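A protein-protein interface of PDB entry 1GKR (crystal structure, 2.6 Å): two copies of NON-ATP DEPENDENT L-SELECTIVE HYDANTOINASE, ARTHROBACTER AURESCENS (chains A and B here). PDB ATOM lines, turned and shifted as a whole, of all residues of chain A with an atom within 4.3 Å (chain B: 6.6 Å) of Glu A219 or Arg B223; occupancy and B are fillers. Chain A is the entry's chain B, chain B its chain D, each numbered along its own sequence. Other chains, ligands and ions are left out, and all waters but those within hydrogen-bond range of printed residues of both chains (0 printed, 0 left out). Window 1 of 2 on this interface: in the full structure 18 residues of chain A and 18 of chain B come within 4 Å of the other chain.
OE1 of Gln A216 sits at hydrogen-bond distance from N of Asn A186.
The side-chain amide nitrogen (ND2) of Asn A186 lies close to the guanidinium group (NH2) of Arg A223 (3.2 Å).
OD1 of Asp B163 is in salt-bridge range of NH1 of Arg B223.
The side-chain amide nitrogen (ND2) of Asn B186 lies within hydrogen-bond range of the side-chain carboxylate (OE1) of Glu B219 (2.9 Å).
The side-chain amide nitrogen (ND2) of Asn B186 sits close to the guanidinium group (NH2) of Arg B223, at 3.2 Å.
NH2 of Arg B223 lies within salt-bridge range of OE1 of Glu B219, 2.8 Å away.
The side-chain amide nitrogen of Asn A186 is in hydrogen-bond range of the side-chain carboxylate of Asp B163.
The side-chain amide oxygen of Gln A222 sits close to the side-chain amide oxygen of Gln B222, at 3.1 Å.
Among the printed residues, pairs that only touch across the chains: Glu A219 with Arg B223 (3.3 Å), Glu A219 with Leu B226 (3.9 Å), Gln A222 with Leu B226 (3.7 Å) and Arg A223 with Glu B219 (3.3 Å).
Glu A219 touches Arg B223, and with the chains exchanged Arg A223 touches Glu B219.
Gln A222 touches its own counterpart, Gln B222.
Positions printed for both chains: 186, 216, 218, 219, 220, 221, 222 and 223.
Printed residues of chain B that touch a printed residue of chain A: Asp B163, Glu B219, Gln B222, Arg B223 and Leu B226.
Hydrophobic or aromatic side chains of chain B within 4 Å of the printed part of chain A: Leu B226.
Of the 10 printed residues of chain A, 4 touch a printed residue of chain B.
Among the printed residues, no Asp or Glu carboxylate lies within 4 Å of a Lys or Arg side-chain nitrogen of the other chain.
Of chain B, only Arg B223 and Leu B226 come within 4 Å of Glu A219.
Arg B223 touches one residue of chain A.
Printed residues of chain A within 4 Å of Asp B163: Asn A186.
Of the printed residues of chain B, Arg A223 touches Glu B219.
Of the printed residues of chain A, Leu B226 touches Glu A219 (3.9 Å) and Gln A222 (3.7 Å).
Of the printed residues of chain B, Asn A186 touches Asp B163 (3.0 Å).
Leu B166 touches none of the printed residues of chain A.
Gln B216 touches none of the printed residues of chain A.
The nearest printed residue of chain B that does not touch Gln A222 is Glu B219 (6.1 Å).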
ATOM      1  N   ASN A 186      -7.981  -8.932 -21.537  1.00  0.00           N
ATOM      2  CA  ASN A 186      -7.310  -7.920 -20.739  1.00  0.00           C
ATOM      3  C   ASN A 186      -6.353  -7.138 -21.641  1.00  0.00           C
ATOM      4  O   ASN A 186      -5.279  -7.616 -22.007  1.00  0.00           O
ATOM      5  CB  ASN A 186      -6.548  -8.561 -19.586  1.00  0.00           C
ATOM      6  CG  ASN A 186      -6.080  -7.540 -18.593  1.00  0.00           C
ATOM      7  OD1 ASN A 186      -5.379  -6.595 -18.952  1.00  0.00           O
ATOM      8  ND2 ASN A 186      -6.473  -7.704 -17.338  1.00  0.00           N
ATOM      9  N   PHE A 215      -5.413 -17.458 -19.909  1.00  0.00           N
ATOM     10  CA  PHE A 215      -5.487 -16.909 -18.565  1.00  0.00           C
ATOM     11  C   PHE A 215      -5.943 -15.457 -18.555  1.00  0.00           C
ATOM     12  O   PHE A 215      -6.641 -15.037 -17.631  1.00  0.00           O
ATOM     13  CB  PHE A 215      -4.161 -17.117 -17.822  1.00  0.00           C
ATOM     14  CG  PHE A 215      -3.206 -15.977 -17.920  1.00  0.00           C
ATOM     15  CD1 PHE A 215      -3.393 -14.827 -17.156  1.00  0.00           C
ATOM     16  CD2 PHE A 215      -2.090 -16.062 -18.741  1.00  0.00           C
ATOM     17  CE1 PHE A 215      -2.482 -13.775 -17.205  1.00  0.00           C
ATOM     18  CE2 PHE A 215      -1.165 -15.014 -18.803  1.00  0.00           C
ATOM     19  CZ  PHE A 215      -1.360 -13.869 -18.034  1.00  0.00           C
ATOM     20  N   GLN A 216      -5.591 -14.687 -19.582  1.00  0.00           N
ATOM     21  CA  GLN A 216      -6.044 -13.302 -19.598  1.00  0.00           C
ATOM     22  C   GLN A 216      -7.474 -13.214 -20.126  1.00  0.00           C
ATOM     23  O   GLN A 216      -8.250 -12.367 -19.682  1.00  0.00           O
ATOM     24  CB  GLN A 216      -5.085 -12.387 -20.388  1.00  0.00           C
ATOM     25  CG  GLN A 216      -4.871 -12.679 -21.857  1.00  0.00           C
ATOM     26  CD  GLN A 216      -5.980 -12.141 -22.726  1.00  0.00           C
ATOM     27  OE1 GLN A 216      -6.523 -11.063 -22.471  1.00  0.00           O
ATOM     28  NE2 GLN A 216      -6.315 -12.878 -23.779  1.00  0.00           N
ATOM     29  N   GLU A 217      -7.847 -14.102 -21.045  1.00  0.00           N
ATOM     30  CA  GLU A 217      -9.213 -14.077 -21.553  1.00  0.00           C
ATOM     31  C   GLU A 217     -10.126 -14.433 -20.392  1.00  0.00           C
ATOM     32  O   GLU A 217     -11.164 -13.808 -20.165  1.00  0.00           O
ATOM     33  CB  GLU A 217      -9.417 -15.107 -22.667  1.00  0.00           C
ATOM     34  CG  GLU A 217     -10.871 -15.243 -23.100  1.00  0.00           C
ATOM     35  CD  GLU A 217     -11.064 -16.264 -24.202  1.00  0.00           C
ATOM     36  OE1 GLU A 217     -10.243 -17.188 -24.326  1.00  0.00           O
ATOM     37  OE2 GLU A 217     -12.050 -16.170 -24.950  1.00  0.00           O
ATOM     38  N   ASN A 218      -9.726 -15.448 -19.646  1.00  0.00           N
ATOM     39  CA  ASN A 218     -10.528 -15.893 -18.528  1.00  0.00           C
ATOM     40  C   ASN A 218     -10.571 -14.905 -17.374  1.00  0.00           C
ATOM     41  O   ASN A 218     -11.551 -14.848 -16.643  1.00  0.00           O
ATOM     42  CB  ASN A 218     -10.042 -17.266 -18.085  1.00  0.00           C
ATOM     43  CG  ASN A 218     -10.382 -18.349 -19.103  1.00  0.00           C
ATOM     44  OD1 ASN A 218      -9.859 -19.461 -19.039  1.00  0.00           O
ATOM     45  ND2 ASN A 218     -11.270 -18.026 -20.041  1.00  0.00           N
ATOM     46  N   GLU A 219      -9.522 -14.111 -17.212  1.00  0.00           N
ATOM     47  CA  GLU A 219      -9.527 -13.120 -16.148  1.00  0.00           C
ATOM     48  C   GLU A 219     -10.595 -12.079 -16.489  1.00  0.00           C
ATOM     49  O   GLU A 219     -11.370 -11.654 -15.627  1.00  0.00           O
ATOM     50  CB  GLU A 219      -8.153 -12.461 -16.040  1.00  0.00           C
ATOM     51  CG  GLU A 219      -8.033 -11.390 -14.963  1.00  0.00           C
ATOM     52  CD  GLU A 219      -8.676 -10.060 -15.360  1.00  0.00           C
ATOM     53  OE1 GLU A 219      -8.470  -9.637 -16.519  1.00  0.00           O
ATOM     54  OE2 GLU A 219      -9.372  -9.431 -14.518  1.00  0.00           O
ATOM     55  N   ALA A 220     -10.645 -11.674 -17.752  1.00  0.00           N
ATOM     56  CA  ALA A 220     -11.617 -10.680 -18.181  1.00  0.00           C
ATOM     57  C   ALA A 220     -13.033 -11.220 -18.002  1.00  0.00           C
ATOM     58  O   ALA A 220     -13.950 -10.489 -17.603  1.00  0.00           O
ATOM     59  CB  ALA A 220     -11.374 -10.305 -19.631  1.00  0.00           C
ATOM     60  N   ILE A 221     -13.221 -12.501 -18.295  1.00  0.00           N
ATOM     61  CA  ILE A 221     -14.539 -13.081 -18.141  1.00  0.00           C
ATOM     62  C   ILE A 221     -14.920 -13.007 -16.658  1.00  0.00           C
ATOM     63  O   ILE A 221     -16.030 -12.592 -16.298  1.00  0.00           O
ATOM     64  CB  ILE A 221     -14.549 -14.535 -18.644  1.00  0.00           C
ATOM     65  CG1 ILE A 221     -14.440 -14.545 -20.170  1.00  0.00           C
ATOM     66  CG2 ILE A 221     -15.812 -15.232 -18.208  1.00  0.00           C
ATOM     67  CD1 ILE A 221     -14.253 -15.943 -20.783  1.00  0.00           C
ATOM     68  N   GLN A 222     -13.976 -13.386 -15.803  1.00  0.00           N
ATOM     69  CA  GLN A 222     -14.174 -13.375 -14.358  1.00  0.00           C
ATOM     70  C   GLN A 222     -14.556 -11.978 -13.870  1.00  0.00           C
ATOM     71  O   GLN A 222     -15.444 -11.818 -13.038  1.00  0.00           O
ATOM     72  CB  GLN A 222     -12.890 -13.815 -13.682  1.00  0.00           C
ATOM     73  CG  GLN A 222     -13.009 -14.153 -12.216  1.00  0.00           C
ATOM     74  CD  GLN A 222     -12.513 -15.574 -11.940  1.00  0.00           C
ATOM     75  OE1 GLN A 222     -12.310 -15.967 -10.788  1.00  0.00           O
ATOM     76  NE2 GLN A 222     -12.320 -16.355 -13.012  1.00  0.00           N
ATOM     77  N   ARG A 223     -13.867 -10.975 -14.404  1.00  0.00           N
ATOM     78  CA  ARG A 223     -14.107  -9.581 -14.055  1.00  0.00           C
ATOM     79  C   ARG A 223     -15.500  -9.103 -14.490  1.00  0.00           C
ATOM     80  O   ARG A 223     -16.215  -8.459 -13.721  1.00  0.00           O
ATOM     81  CB  ARG A 223     -13.043  -8.708 -14.708  1.00  0.00           C
ATOM     82  CG  ARG A 223     -12.668  -7.502 -13.884  1.00  0.00           C
ATOM     83  CD  ARG A 223     -11.816  -6.540 -14.648  1.00  0.00           C
ATOM     84  NE  ARG A 223     -10.896  -7.194 -15.569  1.00  0.00           N
ATOM     85  CZ  ARG A 223     -10.499  -6.633 -16.706  1.00  0.00           C
ATOM     86  NH1 ARG A 223     -10.945  -5.424 -17.028  1.00  0.00           N
ATOM     87  NH2 ARG A 223      -9.680  -7.277 -17.526  1.00  0.00           N
ATOM     88  N   MET B 150      -3.135  -1.124  -6.576  1.00  0.00           N
ATOM     89  CA  MET B 150      -4.068  -1.338  -7.667  1.00  0.00           C
ATOM     90  C   MET B 150      -5.027  -0.163  -7.707  1.00  0.00           C
ATOM     91  O   MET B 150      -5.767   0.010  -8.668  1.00  0.00           O
ATOM     92  CB  MET B 150      -4.825  -2.657  -7.471  1.00  0.00           C
ATOM     93  CG  MET B 150      -3.919  -3.881  -7.581  1.00  0.00           C
ATOM     94  SD  MET B 150      -4.719  -5.457  -7.226  1.00  0.00           S
ATOM     95  CE  MET B 150      -5.866  -5.560  -8.590  1.00  0.00           C
ATOM     96  N   VAL B 161      -0.582   0.593 -10.540  1.00  0.00           N
ATOM     97  CA  VAL B 161      -0.115  -0.088 -11.742  1.00  0.00           C
ATOM     98  C   VAL B 161      -1.302  -0.718 -12.466  1.00  0.00           C
ATOM     99  O   VAL B 161      -2.348  -0.969 -11.864  1.00  0.00           O
ATOM    100  CB  VAL B 161       0.890  -1.201 -11.404  1.00  0.00           C
ATOM    101  CG1 VAL B 161       2.192  -0.603 -10.961  1.00  0.00           C
ATOM    102  CG2 VAL B 161       0.333  -2.086 -10.302  1.00  0.00           C
ATOM    103  N   SER B 162      -1.160  -0.954 -13.758  1.00  0.00           N
ATOM    104  CA  SER B 162      -2.243  -1.594 -14.491  1.00  0.00           C
ATOM    105  C   SER B 162      -2.031  -3.096 -14.338  1.00  0.00           C
ATOM    106  O   SER B 162      -1.006  -3.527 -13.807  1.00  0.00           O
ATOM    107  CB  SER B 162      -2.191  -1.218 -15.962  1.00  0.00           C
ATOM    108  OG  SER B 162      -0.961  -1.607 -16.536  1.00  0.00           O
ATOM    109  N   ASP B 163      -2.977  -3.902 -14.804  1.00  0.00           N
ATOM    110  CA  ASP B 163      -2.817  -5.346 -14.672  1.00  0.00           C
ATOM    111  C   ASP B 163      -1.535  -5.842 -15.347  1.00  0.00           C
ATOM    112  O   ASP B 163      -0.859  -6.718 -14.826  1.00  0.00           O
ATOM    113  CB  ASP B 163      -4.052  -6.077 -15.214  1.00  0.00           C
ATOM    114  CG  ASP B 163      -5.328  -5.668 -14.487  1.00  0.00           C
ATOM    115  OD1 ASP B 163      -5.230  -5.296 -13.308  1.00  0.00           O
ATOM    116  OD2 ASP B 163      -6.431  -5.715 -15.074  1.00  0.00           O
ATOM    117  N   LEU B 166       1.381  -4.750 -13.183  1.00  0.00           N
ATOM    118  CA  LEU B 166       1.299  -5.565 -11.981  1.00  0.00           C
ATOM    119  C   LEU B 166       1.778  -6.983 -12.296  1.00  0.00           C
ATOM    120  O   LEU B 166       2.503  -7.594 -11.511  1.00  0.00           O
ATOM    121  CB  LEU B 166      -0.138  -5.611 -11.463  1.00  0.00           C
ATOM    122  CG  LEU B 166      -0.341  -6.416 -10.170  1.00  0.00           C
ATOM    123  CD1 LEU B 166       0.533  -5.854  -9.053  1.00  0.00           C
ATOM    124  CD2 LEU B 166      -1.793  -6.365  -9.775  1.00  0.00           C
ATOM    125  N   PHE B 170       4.924  -9.035 -10.715  1.00  0.00           N
ATOM    126  CA  PHE B 170       4.769 -10.354 -10.107  1.00  0.00           C
ATOM    127  C   PHE B 170       5.852 -11.288 -10.630  1.00  0.00           C
ATOM    128  O   PHE B 170       6.462 -12.035  -9.856  1.00  0.00           O
ATOM    129  CB  PHE B 170       3.405 -10.949 -10.437  1.00  0.00           C
ATOM    130  CG  PHE B 170       2.296 -10.510  -9.509  1.00  0.00           C
ATOM    131  CD1 PHE B 170       2.452  -9.419  -8.663  1.00  0.00           C
ATOM    132  CD2 PHE B 170       1.075 -11.173  -9.520  1.00  0.00           C
ATOM    133  CE1 PHE B 170       1.402  -8.997  -7.845  1.00  0.00           C
ATOM    134  CE2 PHE B 170       0.029 -10.760  -8.707  1.00  0.00           C
ATOM    135  CZ  PHE B 170       0.194  -9.668  -7.868  1.00  0.00           C
ATOM    136  N   GLU B 185      -7.872  -2.755  -4.559  1.00  0.00           N
ATOM    137  CA  GLU B 185      -9.162  -2.103  -4.758  1.00  0.00           C
ATOM    138  C   GLU B 185      -9.248  -1.781  -6.234  1.00  0.00           C
ATOM    139  O   GLU B 185      -8.244  -1.816  -6.932  1.00  0.00           O
ATOM    140  CB  GLU B 185      -9.298  -0.830  -3.932  1.00  0.00           C
ATOM    141  CG  GLU B 185      -9.488  -1.106  -2.455  1.00  0.00           C
ATOM    142  CD  GLU B 185      -9.994   0.096  -1.707  1.00  0.00           C
ATOM    143  OE1 GLU B 185      -9.168   0.943  -1.290  1.00  0.00           O
ATOM    144  OE2 GLU B 185     -11.228   0.191  -1.555  1.00  0.00           O
ATOM    145  N   ASN B 186     -10.444  -1.498  -6.725  1.00  0.00           N
ATOM    146  CA  ASN B 186     -10.577  -1.174  -8.136  1.00  0.00           C
ATOM    147  C   ASN B 186     -10.654   0.346  -8.286  1.00  0.00           C
ATOM    148  O   ASN B 186     -11.680   0.968  -8.006  1.00  0.00           O
ATOM    149  CB  ASN B 186     -11.821  -1.830  -8.724  1.00  0.00           C
ATOM    150  CG  ASN B 186     -11.839  -1.746 -10.221  1.00  0.00           C
ATOM    151  OD1 ASN B 186     -11.753  -0.659 -10.787  1.00  0.00           O
ATOM    152  ND2 ASN B 186     -11.930  -2.893 -10.880  1.00  0.00           N
ATOM    153  N   GLU B 187      -9.544   0.931  -8.720  1.00  0.00           N
ATOM    154  CA  GLU B 187      -9.434   2.376  -8.886  1.00  0.00           C
ATOM    155  C   GLU B 187     -10.558   3.014  -9.682  1.00  0.00           C
ATOM    156  O   GLU B 187     -11.204   3.961  -9.246  1.00  0.00           O
ATOM    157  CB  GLU B 187      -8.105   2.702  -9.553  1.00  0.00           C
ATOM    158  CG  GLU B 187      -7.957   4.145  -9.929  1.00  0.00           C
ATOM    159  CD  GLU B 187      -6.559   4.655  -9.678  1.00  0.00           C
ATOM    160  OE1 GLU B 187      -6.203   4.863  -8.491  1.00  0.00           O
ATOM    161  OE2 GLU B 187      -5.809   4.839 -10.667  1.00  0.00           O
ATOM    162  N   GLN B 216     -16.100  -4.224  -4.929  1.00  0.00           N
ATOM    163  CA  GLN B 216     -14.944  -3.805  -5.711  1.00  0.00           C
ATOM    164  C   GLN B 216     -13.650  -4.211  -5.012  1.00  0.00           C
ATOM    165  O   GLN B 216     -12.664  -4.542  -5.671  1.00  0.00           O
ATOM    166  CB  GLN B 216     -14.974  -2.295  -6.029  1.00  0.00           C
ATOM    167  CG  GLN B 216     -14.953  -1.325  -4.868  1.00  0.00           C
ATOM    168  CD  GLN B 216     -13.567  -1.105  -4.316  1.00  0.00           C
ATOM    169  OE1 GLN B 216     -12.584  -1.067  -5.060  1.00  0.00           O
ATOM    170  NE2 GLN B 216     -13.476  -0.937  -3.001  1.00  0.00           N
ATOM    171  N   ASN B 218     -13.297  -6.872  -3.253  1.00  0.00           N
ATOM    172  CA  ASN B 218     -13.200  -8.289  -3.519  1.00  0.00           C
ATOM    173  C   ASN B 218     -12.876  -8.618  -4.967  1.00  0.00           C
ATOM    174  O   ASN B 218     -12.254  -9.636  -5.247  1.00  0.00           O
ATOM    175  CB  ASN B 218     -14.477  -8.972  -3.052  1.00  0.00           C
ATOM    176  CG  ASN B 218     -14.590  -8.995  -1.531  1.00  0.00           C
ATOM    177  OD1 ASN B 218     -15.654  -9.275  -0.981  1.00  0.00           O
ATOM    178  ND2 ASN B 218     -13.483  -8.707  -0.849  1.00  0.00           N
ATOM    179  N   GLU B 219     -13.275  -7.759  -5.892  1.00  0.00           N
ATOM    180  CA  GLU B 219     -12.959  -8.004  -7.289  1.00  0.00           C
ATOM    181  C   GLU B 219     -11.441  -7.878  -7.451  1.00  0.00           C
ATOM    182  O   GLU B 219     -10.801  -8.691  -8.122  1.00  0.00           O
ATOM    183  CB  GLU B 219     -13.677  -6.988  -8.176  1.00  0.00           C
ATOM    184  CG  GLU B 219     -13.414  -7.135  -9.670  1.00  0.00           C
ATOM    185  CD  GLU B 219     -12.049  -6.593 -10.098  1.00  0.00           C
ATOM    186  OE1 GLU B 219     -11.685  -5.493  -9.627  1.00  0.00           O
ATOM    187  OE2 GLU B 219     -11.348  -7.251 -10.913  1.00  0.00           O
ATOM    188  N   ALA B 220     -10.863  -6.860  -6.823  1.00  0.00           N
ATOM    189  CA  ALA B 220      -9.429  -6.643  -6.916  1.00  0.00           C
ATOM    190  C   ALA B 220      -8.677  -7.819  -6.299  1.00  0.00           C
ATOM    191  O   ALA B 220      -7.638  -8.254  -6.811  1.00  0.00           O
ATOM    192  CB  ALA B 220      -9.050  -5.350  -6.220  1.00  0.00           C
ATOM    193  N   ILE B 221      -9.199  -8.339  -5.194  1.00  0.00           N
ATOM    194  CA  ILE B 221      -8.543  -9.464  -4.558  1.00  0.00           C
ATOM    195  C   ILE B 221      -8.561 -10.642  -5.538  1.00  0.00           C
ATOM    196  O   ILE B 221      -7.543 -11.310  -5.761  1.00  0.00           O
ATOM    197  CB  ILE B 221      -9.250  -9.825  -3.240  1.00  0.00           C
ATOM    198  CG1 ILE B 221      -8.972  -8.740  -2.200  1.00  0.00           C
ATOM    199  CG2 ILE B 221      -8.773 -11.162  -2.739  1.00  0.00           C
ATOM    200  CD1 ILE B 221      -9.774  -8.890  -0.897  1.00  0.00           C
ATOM    201  N   GLN B 222      -9.724 -10.868  -6.141  1.00  0.00           N
ATOM    202  CA  GLN B 222      -9.914 -11.949  -7.102  1.00  0.00           C
ATOM    203  C   GLN B 222      -8.928 -11.824  -8.264  1.00  0.00           C
ATOM    204  O   GLN B 222      -8.344 -12.808  -8.708  1.00  0.00           O
ATOM    205  CB  GLN B 222     -11.333 -11.892  -7.633  1.00  0.00           C
ATOM    206  CG  GLN B 222     -11.789 -13.109  -8.400  1.00  0.00           C
ATOM    207  CD  GLN B 222     -13.063 -13.695  -7.785  1.00  0.00           C
ATOM    208  OE1 GLN B 222     -13.728 -14.546  -8.384  1.00  0.00           O
ATOM    209  NE2 GLN B 222     -13.405 -13.237  -6.573  1.00  0.00           N
ATOM    210  N   ARG B 223      -8.758 -10.596  -8.744  1.00  0.00           N
ATOM    211  CA  ARG B 223      -7.852 -10.300  -9.845  1.00  0.00           C
ATOM    212  C   ARG B 223      -6.384 -10.562  -9.478  1.00  0.00           C
ATOM    213  O   ARG B 223      -5.640 -11.174 -10.247  1.00  0.00           O
ATOM    214  CB  ARG B 223      -8.020  -8.843 -10.259  1.00  0.00           C
ATOM    215  CG  ARG B 223      -7.817  -8.612 -11.734  1.00  0.00           C
ATOM    216  CD  ARG B 223      -7.743  -7.156 -12.071  1.00  0.00           C
ATOM    217  NE  ARG B 223      -8.613  -6.331 -11.246  1.00  0.00           N
ATOM    218  CZ  ARG B 223      -8.325  -5.072 -10.932  1.00  0.00           C
ATOM    219  NH1 ARG B 223      -7.202  -4.527 -11.387  1.00  0.00           N
ATOM    220  NH2 ARG B 223      -9.136  -4.367 -10.158  1.00  0.00           N
ATOM    221  N   ALA B 224      -5.968 -10.082  -8.312  1.00  0.00           N
ATOM    222  CA  ALA B 224      -4.597 -10.285  -7.867  1.00  0.00           C
ATOM    223  C   ALA B 224      -4.349 -11.774  -7.754  1.00  0.00           C
ATOM    224  O   ALA B 224      -3.303 -12.273  -8.175  1.00  0.00           O
ATOM    225  CB  ALA B 224      -4.380  -9.631  -6.530  1.00  0.00           C
ATOM    226  N   LEU B 225      -5.326 -12.477  -7.187  1.00  0.00           N
ATOM    227  CA  LEU B 225      -5.241 -13.914  -7.018  1.00  0.00           C
ATOM    228  C   LEU B 225      -5.014 -14.637  -8.362  1.00  0.00           C
ATOM    229  O   LEU B 225      -4.128 -15.484  -8.476  1.00  0.00           O
ATOM    230  CB  LEU B 225      -6.517 -14.397  -6.333  1.00  0.00           C
ATOM    231  CG  LEU B 225      -6.456 -14.764  -4.838  1.00  0.00           C
ATOM    232  CD1 LEU B 225      -5.354 -14.044  -4.124  1.00  0.00           C
ATOM    233  CD2 LEU B 225      -7.784 -14.448  -4.195  1.00  0.00           C
ATOM    234  N   LEU B 226      -5.791 -14.282  -9.383  1.00  0.00           N
ATOM    235  CA  LEU B 226      -5.653 -14.896 -10.700  1.00  0.00           C
ATOM    236  C   LEU B 226      -4.294 -14.651 -11.327  1.00  0.00           C
ATOM    237  O   LEU B 226      -3.764 -15.513 -12.031  1.00  0.00           O
ATOM    238  CB  LEU B 226      -6.722 -14.371 -11.647  1.00  0.00           C
ATOM    239  CG  LEU B 226      -7.964 -15.244 -11.798  1.00  0.00           C
ATOM    240  CD1 LEU B 226      -8.448 -15.722 -10.422  1.00  0.00           C
ATOM    241  CD2 LEU B 226      -9.054 -14.444 -12.513  1.00  0.00           C
ATOM    242  N   LEU B 227      -3.732 -13.472 -11.081  1.00  0.00           N
ATOM    243  CA  LEU B 227      -2.428 -13.149 -11.638  1.00  0.00           C
ATOM    244  C   LEU B 227      -1.307 -13.824 -10.871  1.00  0.00           C
ATOM    245  O   LEU B 227      -0.304 -14.194 -11.467  1.00  0.00           O
ATOM    246  CB  LEU B 227      -2.184 -11.632 -11.655  1.00  0.00           C
ATOM    247  CG  LEU B 227      -3.241 -10.762 -12.345  1.00  0.00           C
ATOM    248  CD1 LEU B 227      -2.650  -9.403 -12.647  1.00  0.00           C
ATOM    249  CD2 LEU B 227      -3.685 -11.406 -13.618  1.00  0.00           C
ATOM    250  N   GLN B 228      -1.452 -13.995  -9.561  1.00  0.00           N
ATOM    251  CA  GLN B 228      -0.373 -14.645  -8.833  1.00  0.00           C
ATOM    252  C   GLN B 228      -0.417 -16.125  -9.220  1.00  0.00           C
ATOM    253  O   GLN B 228       0.617 -16.774  -9.409  1.00  0.00           O
ATOM    254  CB  GLN B 228      -0.527 -14.444  -7.320  1.00  0.00           C
ATOM    255  CG  GLN B 228      -1.020 -15.646  -6.583  1.00  0.00           C
ATOM    256  CD  GLN B 228       0.058 -16.668  -6.350  1.00  0.00           C
ATOM    257  OE1 GLN B 228      -0.215 -17.855  -6.329  1.00  0.00           O
ATOM    258  NE2 GLN B 228       1.289 -16.214  -6.164  1.00  0.00           N
